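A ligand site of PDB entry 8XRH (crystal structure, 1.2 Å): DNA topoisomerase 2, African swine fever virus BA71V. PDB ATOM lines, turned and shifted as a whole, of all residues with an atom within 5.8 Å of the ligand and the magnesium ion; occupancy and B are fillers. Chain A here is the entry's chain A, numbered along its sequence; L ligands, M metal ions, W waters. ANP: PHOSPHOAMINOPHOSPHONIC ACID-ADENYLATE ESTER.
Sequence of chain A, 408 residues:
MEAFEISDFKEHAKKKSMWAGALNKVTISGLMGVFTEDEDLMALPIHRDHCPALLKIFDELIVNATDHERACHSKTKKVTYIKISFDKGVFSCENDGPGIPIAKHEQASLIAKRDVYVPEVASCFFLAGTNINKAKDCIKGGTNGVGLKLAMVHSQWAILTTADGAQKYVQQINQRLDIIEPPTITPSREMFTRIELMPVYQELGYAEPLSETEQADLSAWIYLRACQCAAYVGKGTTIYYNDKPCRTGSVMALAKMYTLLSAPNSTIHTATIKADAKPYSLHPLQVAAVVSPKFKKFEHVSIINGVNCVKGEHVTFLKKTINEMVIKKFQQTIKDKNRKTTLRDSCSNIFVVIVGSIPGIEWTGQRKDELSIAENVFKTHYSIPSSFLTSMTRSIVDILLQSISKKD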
ATOM      1  N   GLU A  60       2.823   3.134   4.335  1.00  0.00           N
ATOM      2  CA  GLU A  60       3.318   3.908   5.479  1.00  0.00           C
ATOM      3  C   GLU A  60       2.298   3.906   6.606  1.00  0.00           C
ATOM      4  O   GLU A  60       2.656   3.778   7.789  1.00  0.00           O
ATOM      5  CB  GLU A  60       3.660   5.341   5.062  1.00  0.00           C
ATOM      6  CG  GLU A  60       4.868   5.526   4.130  1.00  0.00           C
ATOM      7  CD  GLU A  60       6.227   5.133   4.697  1.00  0.00           C
ATOM      8  OE1 GLU A  60       6.340   4.770   5.887  1.00  0.00           O
ATOM      9  OE2 GLU A  60       7.205   5.189   3.927  1.00  0.00           O
ATOM     10  N   LEU A  61       1.011   4.023   6.273  1.00  0.00           N
ATOM     11  CA  LEU A  61      -0.018   3.985   7.308  1.00  0.00           C
ATOM     12  C   LEU A  61      -0.116   2.611   7.936  1.00  0.00           C
ATOM     13  O   LEU A  61      -0.240   2.483   9.165  1.00  0.00           O
ATOM     14  CB  LEU A  61      -1.369   4.401   6.740  1.00  0.00           C
ATOM     15  CG  LEU A  61      -1.720   5.888   6.742  1.00  0.00           C
ATOM     16  CD1 LEU A  61      -0.576   6.718   6.268  1.00  0.00           C
ATOM     17  CD2 LEU A  61      -2.968   6.179   5.911  1.00  0.00           C
ATOM     18  N   VAL A  63       2.174   0.196   8.153  1.00  0.00           N
ATOM     19  CA  VAL A  63       3.313  -0.107   9.011  1.00  0.00           C
ATOM     20  C   VAL A  63       3.264   0.718  10.293  1.00  0.00           C
ATOM     21  O   VAL A  63       3.676   0.235  11.347  1.00  0.00           O
ATOM     22  CB  VAL A  63       4.645   0.031   8.255  1.00  0.00           C
ATOM     23  CG1 VAL A  63       5.859  -0.183   9.200  1.00  0.00           C
ATOM     24  CG2 VAL A  63       4.704  -0.933   7.064  1.00  0.00           C
ATOM     25  N   ASN A  64       2.757   1.959  10.244  1.00  0.00           N
ATOM     26  CA  ASN A  64       2.573   2.712  11.486  1.00  0.00           C
ATOM     27  C   ASN A  64       1.651   1.977  12.453  1.00  0.00           C
ATOM     28  O   ASN A  64       1.875   1.965  13.668  1.00  0.00           O
ATOM     29  CB  ASN A  64       2.058   4.120  11.215  1.00  0.00           C
ATOM     30  CG  ASN A  64       3.140   5.041  10.721  1.00  0.00           C
ATOM     31  OD1 ASN A  64       4.329   4.739  10.860  1.00  0.00           O
ATOM     32  ND2 ASN A  64       2.745   6.171  10.140  1.00  0.00           N
ATOM     33  N   ALA A  65       0.578   1.376  11.924  1.00  0.00           N
ATOM     34  CA  ALA A  65      -0.349   0.640  12.771  1.00  0.00           C
ATOM     35  C   ALA A  65       0.274  -0.635  13.333  1.00  0.00           C
ATOM     36  O   ALA A  65       0.099  -0.956  14.513  1.00  0.00           O
ATOM     37  CB  ALA A  65      -1.624   0.317  12.000  1.00  0.00           C
ATOM     38  N   ASP A  67       3.486  -1.075  13.759  1.00  0.00           N
ATOM     39  CA  ASP A  67       4.447  -0.568  14.740  1.00  0.00           C
ATOM     40  C   ASP A  67       3.783  -0.336  16.081  1.00  0.00           C
ATOM     41  O   ASP A  67       4.358  -0.660  17.135  1.00  0.00           O
ATOM     42  CB  ASP A  67       5.073   0.747  14.278  1.00  0.00           C
ATOM     43  CG  ASP A  67       6.092   0.583  13.176  1.00  0.00           C
ATOM     44  OD1 ASP A  67       6.511  -0.552  12.874  1.00  0.00           O
ATOM     45  OD2 ASP A  67       6.535   1.618  12.639  1.00  0.00           O
ATOM     46  N   HIS A  68       2.587   0.256  16.082  1.00  0.00           N
ATOM     47  CA  HIS A  68       1.933   0.545  17.348  1.00  0.00           C
ATOM     48  C   HIS A  68       1.495  -0.749  18.022  1.00  0.00           C
ATOM     49  O   HIS A  68       1.573  -0.881  19.252  1.00  0.00           O
ATOM     50  CB  HIS A  68       0.767   1.496  17.122  1.00  0.00           C
ATOM     51  CG  HIS A  68       0.378   2.270  18.348  1.00  0.00           C
ATOM     52  ND1 HIS A  68       1.262   3.075  19.018  1.00  0.00           N
ATOM     53  CD2 HIS A  68      -0.818   2.390  18.975  1.00  0.00           C
ATOM     54  CE1 HIS A  68       0.635   3.655  20.038  1.00  0.00           C
ATOM     55  NE2 HIS A  68      -0.619   3.253  20.031  1.00  0.00           N
ATOM     56  N   ASN A  95      -6.359   2.113  14.219  1.00  0.00           N
ATOM     57  CA  ASN A  95      -6.021   1.125  15.231  1.00  0.00           C
ATOM     58  C   ASN A  95      -6.427   1.659  16.593  1.00  0.00           C
ATOM     59  O   ASN A  95      -6.506   2.875  16.812  1.00  0.00           O
ATOM     60  CB  ASN A  95      -4.529   0.758  15.235  1.00  0.00           C
ATOM     61  CG  ASN A  95      -3.627   1.973  15.296  1.00  0.00           C
ATOM     62  OD1 ASN A  95      -3.230   2.519  14.271  1.00  0.00           O
ATOM     63  ND2 ASN A  95      -3.248   2.371  16.514  1.00  0.00           N
ATOM     64  N   PRO A  98      -3.324   3.043  22.893  1.00  0.00           N
ATOM     65  CA  PRO A  98      -3.218   4.458  23.270  1.00  0.00           C
ATOM     66  C   PRO A  98      -3.101   5.356  22.044  1.00  0.00           C
ATOM     67  O   PRO A  98      -2.400   5.034  21.077  1.00  0.00           O
ATOM     68  CB  PRO A  98      -1.938   4.500  24.102  1.00  0.00           C
ATOM     69  CG  PRO A  98      -1.884   3.121  24.726  1.00  0.00           C
ATOM     70  CD  PRO A  98      -2.351   2.208  23.628  1.00  0.00           C
ATOM     71  N   GLY A  99      -3.821   6.467  22.067  1.00  0.00           N
ATOM     72  CA  GLY A  99      -3.765   7.418  20.979  1.00  0.00           C
ATOM     73  C   GLY A  99      -2.464   8.194  20.972  1.00  0.00           C
ATOM     74  O   GLY A  99      -1.642   8.132  21.889  1.00  0.00           O
ATOM     75  N   ILE A 100      -2.273   8.949  19.906  1.00  0.00           N
ATOM     76  CA  ILE A 100      -1.175   9.910  19.889  1.00  0.00           C
ATOM     77  C   ILE A 100      -1.455  10.986  20.932  1.00  0.00           C
ATOM     78  O   ILE A 100      -2.581  11.515  20.965  1.00  0.00           O
ATOM     79  CB  ILE A 100      -1.022  10.521  18.499  1.00  0.00           C
ATOM     80  CG1 ILE A 100      -0.661   9.445  17.471  1.00  0.00           C
ATOM     81  CG2 ILE A 100       0.055  11.592  18.501  1.00  0.00           C
ATOM     82  CD1 ILE A 100      -0.630   9.964  16.041  1.00  0.00           C
ATOM     83  N   ALA A 122       3.407  14.767  14.436  1.00  0.00           N
ATOM     84  CA  ALA A 122       3.487  13.416  13.883  1.00  0.00           C
ATOM     85  C   ALA A 122       3.143  13.403  12.405  1.00  0.00           C
ATOM     86  O   ALA A 122       3.723  12.629  11.633  1.00  0.00           O
ATOM     87  CB  ALA A 122       2.549  12.481  14.654  1.00  0.00           C
ATOM     88  N   SER A 123       2.203  14.246  11.978  1.00  0.00           N
ATOM     89  CA  SER A 123       1.662  14.147  10.623  1.00  0.00           C
ATOM     90  C   SER A 123       2.174  15.219   9.678  1.00  0.00           C
ATOM     91  O   SER A 123       2.105  15.018   8.454  1.00  0.00           O
ATOM     92  CB  SER A 123       0.124  14.223  10.669  1.00  0.00           C
ATOM     93  OG  SER A 123      -0.305  15.403  11.332  1.00  0.00           O
ATOM     94  N   ALA A 128      10.375  13.753  12.126  1.00  0.00           N
ATOM     95  CA  ALA A 128       9.803  13.879  13.454  1.00  0.00           C
ATOM     96  C   ALA A 128       8.959  12.669  13.808  1.00  0.00           C
ATOM     97  O   ALA A 128       8.162  12.193  12.990  1.00  0.00           O
ATOM     98  CB  ALA A 128       8.939  15.140  13.579  1.00  0.00           C
ATOM     99  N   GLY A 129       9.137  12.184  15.037  1.00  0.00           N
ATOM    100  CA  GLY A 129       8.414  11.014  15.496  1.00  0.00           C
ATOM    101  C   GLY A 129       9.042  10.494  16.777  1.00  0.00           C
ATOM    102  O   GLY A 129       9.858  11.177  17.410  1.00  0.00           O
ATOM    103  N   THR A 130       8.653   9.278  17.141  1.00  0.00           N
ATOM    104  CA  THR A 130       9.147   8.677  18.376  1.00  0.00           C
ATOM    105  C   THR A 130      10.314   7.727  18.163  1.00  0.00           C
ATOM    106  O   THR A 130      10.752   7.077  19.129  1.00  0.00           O
ATOM    107  CB  THR A 130       8.033   7.946  19.122  1.00  0.00           C
ATOM    108  OG1 THR A 130       7.407   7.014  18.228  1.00  0.00           O
ATOM    109  CG2 THR A 130       6.995   8.937  19.637  1.00  0.00           C
ATOM    110  N   ASN A 131      10.838   7.627  16.938  1.00  0.00           N
ATOM    111  CA  ASN A 131      11.917   6.698  16.611  1.00  0.00           C
ATOM    112  C   ASN A 131      13.176   7.406  16.138  1.00  0.00           C
ATOM    113  O   ASN A 131      14.072   6.763  15.582  1.00  0.00           O
ATOM    114  CB  ASN A 131      11.459   5.659  15.599  1.00  0.00           C
ATOM    115  CG  ASN A 131      10.246   4.897  16.077  1.00  0.00           C
ATOM    116  OD1 ASN A 131      10.328   4.217  17.107  1.00  0.00           O
ATOM    117  ND2 ASN A 131       9.135   5.016  15.388  1.00  0.00           N
ATOM    118  N   LYS A 140      10.261  -2.104  15.601  1.00  0.00           N
ATOM    119  CA  LYS A 140       9.369  -1.316  14.771  1.00  0.00           C
ATOM    120  C   LYS A 140       9.994  -1.127  13.391  1.00  0.00           C
ATOM    121  O   LYS A 140      11.216  -1.032  13.242  1.00  0.00           O
ATOM    122  CB  LYS A 140       9.157   0.066  15.372  1.00  0.00           C
ATOM    123  CG  LYS A 140       8.303   0.066  16.627  1.00  0.00           C
ATOM    124  CD  LYS A 140       7.945   1.500  17.012  1.00  0.00           C
ATOM    125  CE  LYS A 140       6.995   1.522  18.198  1.00  0.00           C
ATOM    126  NZ  LYS A 140       6.735   2.916  18.666  1.00  0.00           N
ATOM    127  N   GLY A 141       9.141  -1.096  12.364  1.00  0.00           N
ATOM    128  CA  GLY A 141       9.623  -0.696  11.047  1.00  0.00           C
ATOM    129  C   GLY A 141       9.988   0.769  11.005  1.00  0.00           C
ATOM    130  O   GLY A 141      11.007   1.152  10.421  1.00  0.00           O
ATOM    131  N   GLY A 142       9.174   1.605  11.639  1.00  0.00           N
ATOM    132  CA  GLY A 142       9.380   3.041  11.577  1.00  0.00           C
ATOM    133  C   GLY A 142      10.717   3.468  12.180  1.00  0.00           C
ATOM    134  O   GLY A 142      11.151   2.970  13.225  1.00  0.00           O
ATOM    135  N   THR A 143      11.366   4.404  11.492  1.00  0.00           N
ATOM    136  CA  THR A 143      12.650   4.892  11.973  1.00  0.00           C
ATOM    137  C   THR A 143      12.891   6.366  11.639  1.00  0.00           C
ATOM    138  O   THR A 143      13.480   7.070  12.446  1.00  0.00           O
ATOM    139  CB  THR A 143      13.798   4.005  11.471  1.00  0.00           C
ATOM    140  OG1 THR A 143      15.046   4.537  11.921  1.00  0.00           O
ATOM    141  CG2 THR A 143      13.802   3.937   9.969  1.00  0.00           C
ATOM    142  N   ASN A 144      12.403   6.859  10.498  1.00  0.00           N
ATOM    143  CA  ASN A 144      12.837   8.170  10.007  1.00  0.00           C
ATOM    144  C   ASN A 144      12.004   9.361  10.439  1.00  0.00           C
ATOM    145  O   ASN A 144      12.495  10.495  10.348  1.00  0.00           O
ATOM    146  CB  ASN A 144      12.967   8.133   8.486  1.00  0.00           C
ATOM    147  CG  ASN A 144      13.926   7.074   8.057  1.00  0.00           C
ATOM    148  OD1 ASN A 144      15.045   7.004   8.591  1.00  0.00           O
ATOM    149  ND2 ASN A 144      13.476   6.185   7.177  1.00  0.00           N
ATOM    150  N   GLY A 145      10.766   9.168  10.897  1.00  0.00           N
ATOM    151  CA  GLY A 145       9.901  10.307  11.144  1.00  0.00           C
ATOM    152  C   GLY A 145       9.467  10.981   9.859  1.00  0.00           C
ATOM    153  O   GLY A 145       9.284  12.211   9.829  1.00  0.00           O
ATOM    154  N   VAL A 146       9.240  10.192   8.804  1.00  0.00           N
ATOM    155  CA  VAL A 146       8.944  10.690   7.472  1.00  0.00           C
ATOM    156  C   VAL A 146       7.635  10.125   6.915  1.00  0.00           C
ATOM    157  O   VAL A 146       6.889  10.845   6.239  1.00  0.00           O
ATOM    158  CB  VAL A 146      10.128  10.375   6.518  1.00  0.00           C
ATOM    159  CG1 VAL A 146       9.747  10.607   5.053  1.00  0.00           C
ATOM    160  CG2 VAL A 146      11.335  11.237   6.887  1.00  0.00           C
ATOM    161  N   GLY A 147       7.350   8.836   7.170  1.00  0.00           N
ATOM    162  CA  GLY A 147       6.331   8.124   6.411  1.00  0.00           C
ATOM    163  C   GLY A 147       4.957   8.781   6.425  1.00  0.00           C
ATOM    164  O   GLY A 147       4.288   8.869   5.385  1.00  0.00           O
ATOM    165  N   LEU A 148       4.494   9.225   7.610  1.00  0.00           N
ATOM    166  CA  LEU A 148       3.142   9.796   7.672  1.00  0.00           C
ATOM    167  C   LEU A 148       3.069  11.108   6.900  1.00  0.00           C
ATOM    168  O   LEU A 148       2.031  11.424   6.303  1.00  0.00           O
ATOM    169  CB  LEU A 148       2.718   9.989   9.127  1.00  0.00           C
ATOM    170  CG  LEU A 148       1.297  10.522   9.354  1.00  0.00           C
ATOM    171  CD1 LEU A 148       0.247   9.721   8.569  1.00  0.00           C
ATOM    172  CD2 LEU A 148       0.993  10.479  10.845  1.00  0.00           C
ATOM    173  N   LYS A 149       4.171  11.867   6.893  1.00  0.00           N
ATOM    174  CA  LYS A 149       4.198  13.105   6.111  1.00  0.00           C
ATOM    175  C   LYS A 149       4.126  12.826   4.621  1.00  0.00           C
ATOM    176  O   LYS A 149       3.540  13.611   3.861  1.00  0.00           O
ATOM    177  CB  LYS A 149       5.447  13.934   6.440  1.00  0.00           C
ATOM    178  CG  LYS A 149       5.316  14.763   7.721  1.00  0.00           C
ATOM    179  CD  LYS A 149       5.180  13.969   9.006  1.00  0.00           C
ATOM    180  CE  LYS A 149       6.354  13.052   9.280  1.00  0.00           C
ATOM    181  NZ  LYS A 149       6.383  12.631  10.727  1.00  0.00           N
ATOM    182  N   THR A 193      -6.314   5.741  16.947  1.00  0.00           N
ATOM    183  CA  THR A 193      -5.692   6.626  15.975  1.00  0.00           C
ATOM    184  C   THR A 193      -6.198   6.229  14.605  1.00  0.00           C
ATOM    185  O   THR A 193      -6.150   5.049  14.230  1.00  0.00           O
ATOM    186  CB  THR A 193      -4.168   6.539  16.025  1.00  0.00           C
ATOM    187  OG1 THR A 193      -3.724   6.851  17.351  1.00  0.00           O
ATOM    188  CG2 THR A 193      -3.517   7.517  15.025  1.00  0.00           C
ATOM    189  N   ILE A 195      -6.238   7.559  10.400  1.00  0.00           N
ATOM    190  CA  ILE A 195      -5.871   8.427   9.291  1.00  0.00           C
ATOM    191  C   ILE A 195      -6.799   8.098   8.144  1.00  0.00           C
ATOM    192  O   ILE A 195      -6.874   6.929   7.742  1.00  0.00           O
ATOM    193  CB  ILE A 195      -4.414   8.204   8.847  1.00  0.00           C
ATOM    194  CG1 ILE A 195      -3.426   8.284  10.020  1.00  0.00           C
ATOM    195  CG2 ILE A 195      -4.062   9.216   7.759  1.00  0.00           C
ATOM    196  CD1 ILE A 195      -3.423   9.593  10.755  1.00  0.00           C
ATOM    197  N   GLN A 366      14.039   5.105   2.602  1.00  0.00           N
ATOM    198  CA  GLN A 366      12.747   5.283   3.253  1.00  0.00           C
ATOM    199  C   GLN A 366      11.755   4.196   2.841  1.00  0.00           C
ATOM    200  O   GLN A 366      10.933   3.768   3.661  1.00  0.00           O
ATOM    201  CB  GLN A 366      12.171   6.672   2.935  1.00  0.00           C
ATOM    202  CG  GLN A 366      10.728   6.880   3.415  1.00  0.00           C
ATOM    203  CD  GLN A 366      10.613   6.954   4.931  1.00  0.00           C
ATOM    204  OE1 GLN A 366      11.525   7.424   5.615  1.00  0.00           O
ATOM    205  NE2 GLN A 366       9.476   6.523   5.472  1.00  0.00           N
ATOM    206  N   LYS A 368      12.211   1.105   2.413  1.00  0.00           N
ATOM    207  CA  LYS A 368      12.426  -0.152   3.141  1.00  0.00           C
ATOM    208  C   LYS A 368      12.205  -1.376   2.244  1.00  0.00           C
ATOM    209  O   LYS A 368      11.546  -2.343   2.612  1.00  0.00           O
ATOM    210  CB  LYS A 368      11.602  -0.214   4.443  1.00  0.00           C
ATOM    211  CG  LYS A 368      11.835   0.988   5.317  1.00  0.00           C
ATOM    212  CD  LYS A 368      10.963   1.061   6.552  1.00  0.00           C
ATOM    213  CE  LYS A 368      11.253   2.328   7.318  1.00  0.00           C
ATOM    214  NZ  LYS A 368      10.409   3.460   6.857  1.00  0.00           N
HETATM  215  PG  ANP L   1       9.168   6.228   9.268  1.00  0.00           P
HETATM  216  O1G ANP L   1       9.413   7.505   8.495  1.00  0.00           O
HETATM  217  O2G ANP L   1      10.312   5.206   9.015  1.00  0.00           O
HETATM  218  O3G ANP L   1       7.764   5.640   9.007  1.00  0.00           O
HETATM  219  PB  ANP L   1       7.945   6.817  11.918  1.00  0.00           P
HETATM  220  O1B ANP L   1       8.478   6.997  13.310  1.00  0.00           O
HETATM  221  O2B ANP L   1       6.865   5.722  11.774  1.00  0.00           O
HETATM  222  N3B ANP L   1       9.290   6.578  10.928  1.00  0.00           N
HETATM  223  PA  ANP L   1       5.911   8.516  10.831  1.00  0.00           P
HETATM  224  O1A ANP L   1       5.401   7.384  10.013  1.00  0.00           O
HETATM  225  O2A ANP L   1       6.009   9.869  10.128  1.00  0.00           O
HETATM  226  O3A ANP L   1       7.401   8.207  11.389  1.00  0.00           O
HETATM  227  O5' ANP L   1       5.029   8.619  12.146  1.00  0.00           O
HETATM  228  C5' ANP L   1       5.330   9.687  13.086  1.00  0.00           C
HETATM  229  C4' ANP L   1       5.031   9.212  14.485  1.00  0.00           C
HETATM  230  O4' ANP L   1       3.607   9.227  14.690  1.00  0.00           O
HETATM  231  C3' ANP L   1       5.451   7.778  14.819  1.00  0.00           C
HETATM  232  O3' ANP L   1       6.812   7.755  15.252  1.00  0.00           O
HETATM  233  C2' ANP L   1       4.494   7.406  15.951  1.00  0.00           C
HETATM  234  O2' ANP L   1       4.975   7.899  17.201  1.00  0.00           O
HETATM  235  C1' ANP L   1       3.221   8.176  15.566  1.00  0.00           C
HETATM  236  N9  ANP L   1       2.206   7.373  14.887  1.00  0.00           N
HETATM  237  C8  ANP L   1       1.993   7.317  13.532  1.00  0.00           C
HETATM  238  N7  ANP L   1       0.999   6.544  13.182  1.00  0.00           N
HETATM  239  C5  ANP L   1       0.522   6.054  14.382  1.00  0.00           C
HETATM  240  C6  ANP L   1      -0.533   5.173  14.693  1.00  0.00           C
HETATM  241  N6  ANP L   1      -1.323   4.594  13.763  1.00  0.00           N
HETATM  242  N1  ANP L   1      -0.758   4.893  15.995  1.00  0.00           N
HETATM  243  C2  ANP L   1       0.023   5.461  16.922  1.00  0.00           C
HETATM  244  N3  ANP L   1       1.058   6.300  16.747  1.00  0.00           N
HETATM  245  C4  ANP L   1       1.245   6.554  15.448  1.00  0.00           C
HETATM  246 MG    MG M   1       6.054   5.349   9.948  1.00  0.00          MG
HETATM  247  O   HOH W   1      -1.593   4.406  10.717  1.00  0.00           O
HETATM  248  O   HOH W   2       6.544   4.590  16.320  1.00  0.00           O
HETATM  249  O   HOH W   3       5.944   4.030  13.733  1.00  0.00           O
HETATM  250  O   HOH W   4       6.589   3.266  10.060  1.00  0.00           O
HETATM  251  O   HOH W   5       3.371   4.063  14.922  1.00  0.00           O
HETATM  252  O   HOH W   6      10.386   8.725  14.251  1.00  0.00           O
HETATM  253  O   HOH W   7      -3.984   3.543  11.853  1.00  0.00           O
HETATM  254  O   HOH W   8       7.452   2.702   7.302  1.00  0.00           O
HETATM  255  O   HOH W   9       2.040   7.359  19.213  1.00  0.00           O
HETATM  256  O   HOH W  10      -0.074   6.738  10.535  1.00  0.00           O
HETATM  257  O   HOH W  11       5.075   5.051   8.162  1.00  0.00           O
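N of Asn 144 is in hydrogen-bond range of O2G of the ligand (3.1 Å). The backbone NH of Gly 145 sits at hydrogen-bond distance from an oxygen (O1G) of the ligand (3.2 Å). OG1 of Thr 130 lies within hydrogen-bond range of O2' of the ligand (2.8 Å). The side-chain amino group (NZ) of Lys 368 lies within salt-bridge range of an oxygen (O2G) of the ligand (2.8 Å). OD1 of Asn 95 sits at hydrogen-bond distance from N6 of the ligand (2.9 Å). NE2 of Gln 366 lies within hydrogen-bond range of O1G of the ligand. O1G of the ligand is in hydrogen-bond range of N of Gly 147 (2.8 Å). N of Thr 143 is in hydrogen-bond range of O2G of the ligand, at 2.8 Å. NZ of Lys 149 is in salt-bridge range of O2A of the ligand, at 2.9 Å. The backbone NH (N) of Leu 148 sits at hydrogen-bond distance from an oxygen (O2A) of the ligand (3.0 Å). An oxygen (O1B) of the ligand is in hydrogen-bond range of the side-chain amide nitrogen (ND2) of Asn 131 (2.9 Å). An oxygen (O1G) of the ligand is in hydrogen-bond range of the backbone NH (N) of Val 146 (2.7 Å). An oxygen (O3') of the ligand lies within hydrogen-bond range of the backbone NH (N) of Thr 130.
One residue has an atom within 4 Å of the magnesium ion: Asn 64.
The magnesium ion is bound by an oxygen (O3G) of the ligand, 2.0 Å away. O2B of the ligand is bound to the magnesium ion (2.0 Å). The magnesium ion is bound by OD1 of Asn 64 (2.0 Å). The magnesium ion is bound by water W11 (2.1 Å). The magnesium ion is bound by O1A of the ligand. Water W4 binds the magnesium ion, 2.2 Å away. The magnesium ion has six donor atoms within binding distance.
NE2 of Gln 366 lies within hydrogen-bond range of OE2 of Glu 60 (3.1 Å). A ring nitrogen (NE2) of His 68 is in hydrogen-bond range of the backbone carbonyl oxygen (O) of Pro 98, at 2.7 Å. N of Thr 193 lies within hydrogen-bond range of O of Asn 95. The side-chain amino group of Lys 149 is in hydrogen-bond range of the backbone carbonyl oxygen of Gly 145, at 3.1 Å. O of Ala 122 is in hydrogen-bond range of NZ of Lys 149 (2.8 Å). The backbone carbonyl oxygen (O) of Glu 60 sits close to the side-chain amide nitrogen (ND2) of Asn 64, 3.4 Å away. NZ of Lys 368 sits at hydrogen-bond distance from O of Gln 366 (3.3 Å). OE1 of Gln 366 is in hydrogen-bond range of ND2 of Asn 144.
Water W4 lies within hydrogen-bond range of OD2 of Asp 67 (3.1 Å) and N of Gly 142 (3.5 Å). Water W11 bridges the side-chain carboxylate of Glu 60 and the side-chain amide nitrogen of Asn 64. Water W10 lies within hydrogen-bond range of N7 of the ligand (2.9 Å) and ND2 of Asn 64 (2.9 Å). Water W1 lies within hydrogen-bond range of O of Leu 61 and N6 of the ligand. Water W2 lies within hydrogen-bond range of the side-chain amide nitrogen of Asn 131 (2.8 Å), the side-chain amino group of Lys 140 (2.9 Å), the side-chain hydroxyl of Thr 130 (3.2 Å) and an oxygen (O3') of the ligand (3.4 Å). Water W8 bridges the side-chain carboxylate of Glu 60 (2.7 Å) and the side-chain amino group of Lys 368 (3.1 Å).
OE1 of Glu 60 touches O3G of the ligand, 3.5 Å away. His 68 touches the ligand. Ile 100 touches the ligand. CB of Ala 122 touches O4' of the ligand, at 3.4 Å. Ala 128 touches the ligand (O to C5', 3.8 Å). Gly 129 touches the ligand. Gly 142 touches the ligand (CA to O2G, 3.5 Å). CB of Thr 193 touches N1 of the ligand, at 3.8 Å. Hydrophobic or aromatic side chains within 4 Å of the ligand: His 68, Ile 100, Ala 122, Val 146 and Leu 148. The nearest printed residue that does not touch the ligand is Ala 65 (4.2 Å).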
